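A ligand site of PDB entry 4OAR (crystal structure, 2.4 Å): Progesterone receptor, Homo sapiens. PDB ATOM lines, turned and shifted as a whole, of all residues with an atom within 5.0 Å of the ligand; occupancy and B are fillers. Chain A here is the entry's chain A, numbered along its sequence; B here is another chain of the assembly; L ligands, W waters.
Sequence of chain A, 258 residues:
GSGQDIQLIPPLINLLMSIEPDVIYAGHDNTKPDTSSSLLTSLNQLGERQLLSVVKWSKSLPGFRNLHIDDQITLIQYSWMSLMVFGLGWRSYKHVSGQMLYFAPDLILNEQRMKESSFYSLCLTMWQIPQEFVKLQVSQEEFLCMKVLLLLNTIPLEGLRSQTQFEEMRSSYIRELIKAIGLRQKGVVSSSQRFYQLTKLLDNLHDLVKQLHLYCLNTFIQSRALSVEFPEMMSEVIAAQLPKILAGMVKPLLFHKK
SG of Cys 216 sits close to O2 of the ligand (3.7 Å). An oxygen (O1) of the ligand lies within hydrogen-bond range of the guanidinium group (NH2) of Arg 91. The side-chain hydroxyl (OG1) of Thr 219 is in hydrogen-bond range of an oxygen (O3) of the ligand, 3.1 Å away. The side-chain amide nitrogen of Gln 50 is in hydrogen-bond range of an oxygen (O1) of the ligand.
O of Phe 103 sits at hydrogen-bond distance from NH2 of Arg 91 (3.1 Å). The backbone carbonyl oxygen of Tyr 215 sits at hydrogen-bond distance from the side-chain hydroxyl of Thr 219, 2.8 Å away.
Merely in contact with the ligand: Leu 40 (3.7 Å), Leu 43 (3.6 Å), Asn 44 (3.4 Å), Leu 46 (3.7 Å), Gly 47 (3.5 Å), Glu 48 (3.7 Å), Trp 80 (3.7 Å), Met 84 (3.8 Å), Phe 103 (3.8 Å), Phe 119 (3.7 Å), Leu 122 (3.6 Å) and Met 126 (3.8 Å). Hydrophobic or aromatic side chains within 4 Å of the ligand: Leu 40, Leu 46, Trp 80, Met 84, Phe 103, Phe 119, Leu 122 and Met 126. Of the 23 residues printed, 16 come within 4 Å of the ligand. The nearest printed residue that does not touch the ligand is Tyr 215 (4.1 Å).
Water W1 lies within hydrogen-bond range of the side-chain amide nitrogen of Gln 50 (2.7 Å), the backbone carbonyl oxygen of Met 84 (2.9 Å), an oxygen (O1) of the ligand (2.9 Å) and the guanidinium group of Arg 91 (3.1 Å).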
ATOM      1  N   LEU A  40       8.646  19.490  21.250  1.00  0.00           N
ATOM      2  CA  LEU A  40       7.939  19.657  19.983  1.00  0.00           C
ATOM      3  C   LEU A  40       7.308  18.334  19.530  1.00  0.00           C
ATOM      4  O   LEU A  40       6.244  18.344  18.896  1.00  0.00           O
ATOM      5  CB  LEU A  40       8.883  20.186  18.898  1.00  0.00           C
ATOM      6  CG  LEU A  40       9.162  21.689  18.929  1.00  0.00           C
ATOM      7  CD1 LEU A  40      10.560  21.979  18.384  1.00  0.00           C
ATOM      8  CD2 LEU A  40       8.105  22.430  18.113  1.00  0.00           C
ATOM      9  N   LEU A  43       4.076  17.809  21.560  1.00  0.00           N
ATOM     10  CA  LEU A  43       2.999  18.669  21.082  1.00  0.00           C
ATOM     11  C   LEU A  43       2.360  18.158  19.795  1.00  0.00           C
ATOM     12  O   LEU A  43       1.135  18.236  19.638  1.00  0.00           O
ATOM     13  CB  LEU A  43       3.512  20.103  20.887  1.00  0.00           C
ATOM     14  CG  LEU A  43       3.844  20.850  22.171  1.00  0.00           C
ATOM     15  CD1 LEU A  43       4.583  22.154  21.849  1.00  0.00           C
ATOM     16  CD2 LEU A  43       2.562  21.108  22.963  1.00  0.00           C
ATOM     17  N   ASN A  44       3.170  17.659  18.877  1.00  0.00           N
ATOM     18  CA  ASN A  44       2.655  17.123  17.627  1.00  0.00           C
ATOM     19  C   ASN A  44       1.814  15.878  17.881  1.00  0.00           C
ATOM     20  O   ASN A  44       0.754  15.720  17.284  1.00  0.00           O
ATOM     21  CB  ASN A  44       3.793  16.833  16.644  1.00  0.00           C
ATOM     22  CG  ASN A  44       4.371  18.109  16.039  1.00  0.00           C
ATOM     23  OD1 ASN A  44       3.953  19.220  16.368  1.00  0.00           O
ATOM     24  ND2 ASN A  44       5.337  17.956  15.144  1.00  0.00           N
ATOM     25  N   LEU A  46       0.207  15.234  20.603  1.00  0.00           N
ATOM     26  CA  LEU A  46      -1.001  15.685  21.271  1.00  0.00           C
ATOM     27  C   LEU A  46      -1.960  16.274  20.249  1.00  0.00           C
ATOM     28  O   LEU A  46      -3.158  16.019  20.293  1.00  0.00           O
ATOM     29  CB  LEU A  46      -0.650  16.710  22.364  1.00  0.00           C
ATOM     30  CG  LEU A  46      -1.767  17.145  23.310  1.00  0.00           C
ATOM     31  CD1 LEU A  46      -2.319  15.942  24.043  1.00  0.00           C
ATOM     32  CD2 LEU A  46      -1.244  18.171  24.290  1.00  0.00           C
ATOM     33  N   GLY A  47      -1.412  17.038  19.312  1.00  0.00           N
ATOM     34  CA  GLY A  47      -2.218  17.657  18.269  1.00  0.00           C
ATOM     35  C   GLY A  47      -2.948  16.636  17.414  1.00  0.00           C
ATOM     36  O   GLY A  47      -4.113  16.838  17.088  1.00  0.00           O
ATOM     37  N   GLU A  48      -2.257  15.551  17.054  1.00  0.00           N
ATOM     38  CA  GLU A  48      -2.844  14.483  16.243  1.00  0.00           C
ATOM     39  C   GLU A  48      -3.997  13.829  16.998  1.00  0.00           C
ATOM     40  O   GLU A  48      -5.069  13.597  16.437  1.00  0.00           O
ATOM     41  CB  GLU A  48      -1.805  13.423  15.885  1.00  0.00           C
ATOM     42  CG  GLU A  48      -0.617  13.960  15.073  1.00  0.00           C
ATOM     43  CD  GLU A  48       0.363  12.876  14.611  1.00  0.00           C
ATOM     44  OE1 GLU A  48       0.387  12.586  13.396  1.00  0.00           O
ATOM     45  OE2 GLU A  48       1.110  12.335  15.445  1.00  0.00           O
ATOM     46  N   GLN A  50      -5.733  15.173  19.501  1.00  0.00           N
ATOM     47  CA  GLN A  50      -6.789  16.160  19.687  1.00  0.00           C
ATOM     48  C   GLN A  50      -7.630  16.393  18.428  1.00  0.00           C
ATOM     49  O   GLN A  50      -8.800  16.759  18.517  1.00  0.00           O
ATOM     50  CB  GLN A  50      -6.232  17.486  20.224  1.00  0.00           C
ATOM     51  CG  GLN A  50      -5.948  17.431  21.730  1.00  0.00           C
ATOM     52  CD  GLN A  50      -5.465  18.754  22.315  1.00  0.00           C
ATOM     53  OE1 GLN A  50      -5.200  18.855  23.506  1.00  0.00           O
ATOM     54  NE2 GLN A  50      -5.354  19.775  21.462  1.00  0.00           N
ATOM     55  N   LEU A  51      -7.017  16.163  17.259  1.00  0.00           N
ATOM     56  CA  LEU A  51      -7.715  16.340  15.997  1.00  0.00           C
ATOM     57  C   LEU A  51      -8.806  15.270  15.857  1.00  0.00           C
ATOM     58  O   LEU A  51      -9.953  15.578  15.503  1.00  0.00           O
ATOM     59  CB  LEU A  51      -6.742  16.235  14.824  1.00  0.00           C
ATOM     60  CG  LEU A  51      -7.350  16.467  13.421  1.00  0.00           C
ATOM     61  CD1 LEU A  51      -7.815  17.908  13.263  1.00  0.00           C
ATOM     62  CD2 LEU A  51      -6.328  16.123  12.364  1.00  0.00           C
ATOM     63  N   TRP A  80     -10.166  23.587  13.336  1.00  0.00           N
ATOM     64  CA  TRP A  80      -9.335  22.821  14.270  1.00  0.00           C
ATOM     65  C   TRP A  80      -8.336  23.607  15.112  1.00  0.00           C
ATOM     66  O   TRP A  80      -8.212  23.335  16.311  1.00  0.00           O
ATOM     67  CB  TRP A  80      -8.673  21.598  13.605  1.00  0.00           C
ATOM     68  CG  TRP A  80      -7.655  21.890  12.550  1.00  0.00           C
ATOM     69  CD1 TRP A  80      -7.848  21.936  11.206  1.00  0.00           C
ATOM     70  CD2 TRP A  80      -6.252  22.151  12.751  1.00  0.00           C
ATOM     71  NE1 TRP A  80      -6.659  22.208  10.558  1.00  0.00           N
ATOM     72  CE2 TRP A  80      -5.667  22.347  11.495  1.00  0.00           C
ATOM     73  CE3 TRP A  80      -5.441  22.237  13.899  1.00  0.00           C
ATOM     74  CZ2 TRP A  80      -4.301  22.622  11.329  1.00  0.00           C
ATOM     75  CZ3 TRP A  80      -4.089  22.513  13.734  1.00  0.00           C
ATOM     76  CH2 TRP A  80      -3.529  22.699  12.462  1.00  0.00           C
ATOM     77  N   MET A  81      -7.689  24.623  14.529  1.00  0.00           N
ATOM     78  CA  MET A  81      -6.720  25.442  15.261  1.00  0.00           C
ATOM     79  C   MET A  81      -7.398  26.247  16.352  1.00  0.00           C
ATOM     80  O   MET A  81      -6.946  26.296  17.481  1.00  0.00           O
ATOM     81  CB  MET A  81      -5.992  26.416  14.340  1.00  0.00           C
ATOM     82  CG  MET A  81      -4.887  27.214  14.990  1.00  0.00           C
ATOM     83  SD  MET A  81      -3.585  26.270  15.791  1.00  0.00           S
ATOM     84  CE  MET A  81      -2.614  25.892  14.369  1.00  0.00           C
ATOM     85  N   MET A  84      -8.647  24.024  19.201  1.00  0.00           N
ATOM     86  CA  MET A  84      -7.555  23.529  20.041  1.00  0.00           C
ATOM     87  C   MET A  84      -6.988  24.587  20.994  1.00  0.00           C
ATOM     88  O   MET A  84      -6.728  24.285  22.163  1.00  0.00           O
ATOM     89  CB  MET A  84      -6.413  22.986  19.182  1.00  0.00           C
ATOM     90  CG  MET A  84      -6.713  21.650  18.522  1.00  0.00           C
ATOM     91  SD  MET A  84      -5.270  20.958  17.688  1.00  0.00           S
ATOM     92  CE  MET A  84      -5.887  19.333  17.265  1.00  0.00           C
ATOM     93  N   VAL A  85      -6.825  25.817  20.510  1.00  0.00           N
ATOM     94  CA  VAL A  85      -6.307  26.870  21.363  1.00  0.00           C
ATOM     95  C   VAL A  85      -7.371  27.399  22.350  1.00  0.00           C
ATOM     96  O   VAL A  85      -7.032  27.937  23.401  1.00  0.00           O
ATOM     97  CB  VAL A  85      -5.691  28.040  20.546  1.00  0.00           C
ATOM     98  CG1 VAL A  85      -6.769  28.995  20.029  1.00  0.00           C
ATOM     99  CG2 VAL A  85      -4.661  28.791  21.383  1.00  0.00           C
ATOM    100  N   LEU A  88      -7.401  24.788  25.130  1.00  0.00           N
ATOM    101  CA  LEU A  88      -6.207  24.995  25.945  1.00  0.00           C
ATOM    102  C   LEU A  88      -6.510  26.155  26.901  1.00  0.00           C
ATOM    103  O   LEU A  88      -6.172  26.104  28.087  1.00  0.00           O
ATOM    104  CB  LEU A  88      -5.017  25.360  25.040  1.00  0.00           C
ATOM    105  CG  LEU A  88      -3.727  25.836  25.713  1.00  0.00           C
ATOM    106  CD1 LEU A  88      -3.062  24.665  26.425  1.00  0.00           C
ATOM    107  CD2 LEU A  88      -2.780  26.456  24.669  1.00  0.00           C
ATOM    108  N   ARG A  91      -8.806  24.841  29.861  1.00  0.00           N
ATOM    109  CA  ARG A  91      -8.086  23.985  30.799  1.00  0.00           C
ATOM    110  C   ARG A  91      -7.110  24.789  31.671  1.00  0.00           C
ATOM    111  O   ARG A  91      -7.052  24.599  32.887  1.00  0.00           O
ATOM    112  CB  ARG A  91      -7.318  22.879  30.054  1.00  0.00           C
ATOM    113  CG  ARG A  91      -8.212  21.849  29.384  1.00  0.00           C
ATOM    114  CD  ARG A  91      -7.421  20.651  28.862  1.00  0.00           C
ATOM    115  NE  ARG A  91      -6.376  21.043  27.917  1.00  0.00           N
ATOM    116  CZ  ARG A  91      -6.568  21.230  26.612  1.00  0.00           C
ATOM    117  NH1 ARG A  91      -7.776  21.079  26.080  1.00  0.00           N
ATOM    118  NH2 ARG A  91      -5.540  21.553  25.827  1.00  0.00           N
ATOM    119  N   PHE A 103      -1.563  22.134  28.597  1.00  0.00           N
ATOM    120  CA  PHE A 103      -1.794  21.413  27.345  1.00  0.00           C
ATOM    121  C   PHE A 103      -2.458  20.072  27.618  1.00  0.00           C
ATOM    122  O   PHE A 103      -3.379  19.660  26.901  1.00  0.00           O
ATOM    123  CB  PHE A 103      -0.465  21.208  26.587  1.00  0.00           C
ATOM    124  CG  PHE A 103       0.087  22.464  25.968  1.00  0.00           C
ATOM    125  CD1 PHE A 103       0.996  23.251  26.664  1.00  0.00           C
ATOM    126  CD2 PHE A 103      -0.311  22.862  24.693  1.00  0.00           C
ATOM    127  CE1 PHE A 103       1.527  24.415  26.093  1.00  0.00           C
ATOM    128  CE2 PHE A 103       0.211  24.034  24.101  1.00  0.00           C
ATOM    129  CZ  PHE A 103       1.128  24.811  24.805  1.00  0.00           C
ATOM    130  N   PHE A 119      10.030  29.222  21.695  1.00  0.00           N
ATOM    131  CA  PHE A 119       8.764  29.751  21.202  1.00  0.00           C
ATOM    132  C   PHE A 119       7.983  30.483  22.285  1.00  0.00           C
ATOM    133  O   PHE A 119       6.764  30.320  22.417  1.00  0.00           O
ATOM    134  CB  PHE A 119       7.908  28.643  20.570  1.00  0.00           C
ATOM    135  CG  PHE A 119       7.604  27.494  21.503  1.00  0.00           C
ATOM    136  CD1 PHE A 119       6.491  27.526  22.332  1.00  0.00           C
ATOM    137  CD2 PHE A 119       8.426  26.379  21.535  1.00  0.00           C
ATOM    138  CE1 PHE A 119       6.182  26.464  23.185  1.00  0.00           C
ATOM    139  CE2 PHE A 119       8.135  25.304  22.380  1.00  0.00           C
ATOM    140  CZ  PHE A 119       7.011  25.357  23.207  1.00  0.00           C
ATOM    141  N   LEU A 122       5.135  32.619  20.879  1.00  0.00           N
ATOM    142  CA  LEU A 122       3.917  31.855  20.610  1.00  0.00           C
ATOM    143  C   LEU A 122       3.155  31.627  21.919  1.00  0.00           C
ATOM    144  O   LEU A 122       1.933  31.839  21.985  1.00  0.00           O
ATOM    145  CB  LEU A 122       4.265  30.507  19.971  1.00  0.00           C
ATOM    146  CG  LEU A 122       3.117  29.520  19.752  1.00  0.00           C
ATOM    147  CD1 LEU A 122       2.223  29.998  18.618  1.00  0.00           C
ATOM    148  CD2 LEU A 122       3.659  28.132  19.440  1.00  0.00           C
ATOM    149  N   MET A 126      -0.807  32.581  22.793  1.00  0.00           N
ATOM    150  CA  MET A 126      -1.812  31.632  23.266  1.00  0.00           C
ATOM    151  C   MET A 126      -2.292  31.925  24.673  1.00  0.00           C
ATOM    152  O   MET A 126      -3.475  31.752  24.990  1.00  0.00           O
ATOM    153  CB  MET A 126      -1.283  30.189  23.190  1.00  0.00           C
ATOM    154  CG  MET A 126      -1.060  29.696  21.771  1.00  0.00           C
ATOM    155  SD  MET A 126      -0.533  27.974  21.679  1.00  0.00           S
ATOM    156  CE  MET A 126       1.071  28.068  22.504  1.00  0.00           C
ATOM    157  N   LEU A 212      -1.173  31.875  14.741  1.00  0.00           N
ATOM    158  CA  LEU A 212      -0.819  30.484  15.045  1.00  0.00           C
ATOM    159  C   LEU A 212      -0.494  29.691  13.773  1.00  0.00           C
ATOM    160  O   LEU A 212       0.419  28.867  13.768  1.00  0.00           O
ATOM    161  CB  LEU A 212      -1.937  29.783  15.839  1.00  0.00           C
ATOM    162  CG  LEU A 212      -2.343  30.366  17.197  1.00  0.00           C
ATOM    163  CD1 LEU A 212      -3.328  29.450  17.907  1.00  0.00           C
ATOM    164  CD2 LEU A 212      -1.135  30.563  18.077  1.00  0.00           C
ATOM    165  N   TYR A 215       3.027  30.652  12.615  1.00  0.00           N
ATOM    166  CA  TYR A 215       4.029  30.006  13.466  1.00  0.00           C
ATOM    167  C   TYR A 215       4.238  28.575  13.015  1.00  0.00           C
ATOM    168  O   TYR A 215       5.374  28.118  12.861  1.00  0.00           O
ATOM    169  CB  TYR A 215       3.581  29.999  14.929  1.00  0.00           C
ATOM    170  CG  TYR A 215       4.010  31.221  15.706  1.00  0.00           C
ATOM    171  CD1 TYR A 215       5.351  31.388  16.078  1.00  0.00           C
ATOM    172  CD2 TYR A 215       3.086  32.201  16.084  1.00  0.00           C
ATOM    173  CE1 TYR A 215       5.756  32.522  16.810  1.00  0.00           C
ATOM    174  CE2 TYR A 215       3.474  33.324  16.806  1.00  0.00           C
ATOM    175  CZ  TYR A 215       4.813  33.488  17.164  1.00  0.00           C
ATOM    176  OH  TYR A 215       5.206  34.617  17.862  1.00  0.00           O
ATOM    177  N   CYS A 216       3.128  27.888  12.781  1.00  0.00           N
ATOM    178  CA  CYS A 216       3.138  26.512  12.343  1.00  0.00           C
ATOM    179  C   CYS A 216       3.873  26.400  11.004  1.00  0.00           C
ATOM    180  O   CYS A 216       4.723  25.520  10.837  1.00  0.00           O
ATOM    181  CB  CYS A 216       1.701  25.990  12.201  1.00  0.00           C
ATOM    182  SG  CYS A 216       1.603  24.309  11.558  1.00  0.00           S
ATOM    183  N   THR A 219       7.606  27.150  11.559  1.00  0.00           N
ATOM    184  CA  THR A 219       8.284  26.098  12.313  1.00  0.00           C
ATOM    185  C   THR A 219       8.572  24.913  11.377  1.00  0.00           C
ATOM    186  O   THR A 219       9.550  24.198  11.547  1.00  0.00           O
ATOM    187  CB  THR A 219       7.427  25.633  13.512  1.00  0.00           C
ATOM    188  OG1 THR A 219       7.215  26.729  14.401  1.00  0.00           O
ATOM    189  CG2 THR A 219       8.117  24.509  14.270  1.00  0.00           C
ATOM    190  N   LEU B   5      -4.106  16.288   6.033  1.00  0.00           N
ATOM    191  CA  LEU B   5      -5.157  16.451   7.040  1.00  0.00           C
ATOM    192  C   LEU B   5      -6.553  16.212   6.479  1.00  0.00           C
ATOM    193  O   LEU B   5      -7.370  15.552   7.118  1.00  0.00           O
ATOM    194  CB  LEU B   5      -5.076  17.828   7.690  1.00  0.00           C
ATOM    195  CG  LEU B   5      -3.858  18.080   8.588  1.00  0.00           C
ATOM    196  CD1 LEU B   5      -4.019  19.404   9.312  1.00  0.00           C
ATOM    197  CD2 LEU B   5      -3.708  16.936   9.582  1.00  0.00           C
HETATM  198  C1  LIG L   1      -1.476  20.963  20.400  1.00  0.00           C
HETATM  199  C2  LIG L   1      -2.186  20.688  21.710  1.00  0.00           C
HETATM  200  C3  LIG L   1      -3.133  21.869  22.273  1.00  0.00           C
HETATM  201  C4  LIG L   1      -3.199  23.050  21.564  1.00  0.00           C
HETATM  202  C5  LIG L   1      -2.453  23.297  20.392  1.00  0.00           C
HETATM  203  C6  LIG L   1      -2.663  24.671  19.764  1.00  0.00           C
HETATM  204  C7  LIG L   1      -1.392  25.259  19.156  1.00  0.00           C
HETATM  205  C8  LIG L   1      -0.550  24.278  18.355  1.00  0.00           C
HETATM  206  C9  LIG L   1      -0.487  22.781  18.853  1.00  0.00           C
HETATM  207  C10 LIG L   1      -1.462  22.354  19.874  1.00  0.00           C
HETATM  208  C11 LIG L   1       0.592  21.807  18.218  1.00  0.00           C
HETATM  209  C12 LIG L   1       1.664  22.457  17.506  1.00  0.00           C
HETATM  210  C13 LIG L   1       1.456  23.798  16.761  1.00  0.00           C
HETATM  211  C14 LIG L   1       0.746  24.763  17.653  1.00  0.00           C
HETATM  212  C15 LIG L   1       0.906  26.135  17.000  1.00  0.00           C
HETATM  213  C16 LIG L   1       2.246  26.004  16.256  1.00  0.00           C
HETATM  214  C17 LIG L   1       2.746  24.549  16.470  1.00  0.00           C
HETATM  215  C18 LIG L   1       0.726  23.498  15.450  1.00  0.00           C
HETATM  216  C19 LIG L   1       3.791  24.034  15.439  1.00  0.00           C
HETATM  217  C20 LIG L   1       4.619  22.780  15.655  1.00  0.00           C
HETATM  218  O1  LIG L   1      -3.818  21.645  23.331  1.00  0.00           O
HETATM  219  O2  LIG L   1       4.016  24.609  14.410  1.00  0.00           O
HETATM  220  C21 LIG L   1      -0.119  20.838  17.169  1.00  0.00           C
HETATM  221  C22 LIG L   1      -1.450  21.012  16.815  1.00  0.00           C
HETATM  222  C23 LIG L   1      -2.049  20.230  15.839  1.00  0.00           C
HETATM  223  C24 LIG L   1      -1.303  19.238  15.200  1.00  0.00           C
HETATM  224  C25 LIG L   1       0.022  19.040  15.530  1.00  0.00           C
HETATM  225  C26 LIG L   1       0.617  19.844  16.510  1.00  0.00           C
HETATM  226  N1  LIG L   1      -1.906  18.434  14.265  1.00  0.00           N
HETATM  227  C27 LIG L   1      -3.168  18.657  13.783  1.00  0.00           C
HETATM  228  C28 LIG L   1      -1.296  17.337  13.745  1.00  0.00           C
HETATM  229  C29 LIG L   1       5.823  25.224  19.133  1.00  0.00           C
HETATM  230  C30 LIG L   1       5.104  25.142  17.796  1.00  0.00           C
HETATM  231  O3  LIG L   1       5.688  25.626  16.809  1.00  0.00           O
HETATM  232  O4  LIG L   1       3.761  24.578  17.648  1.00  0.00           O
HETATM  233  O   HOH W   1      -6.733  21.540  22.952  1.00  0.00           O
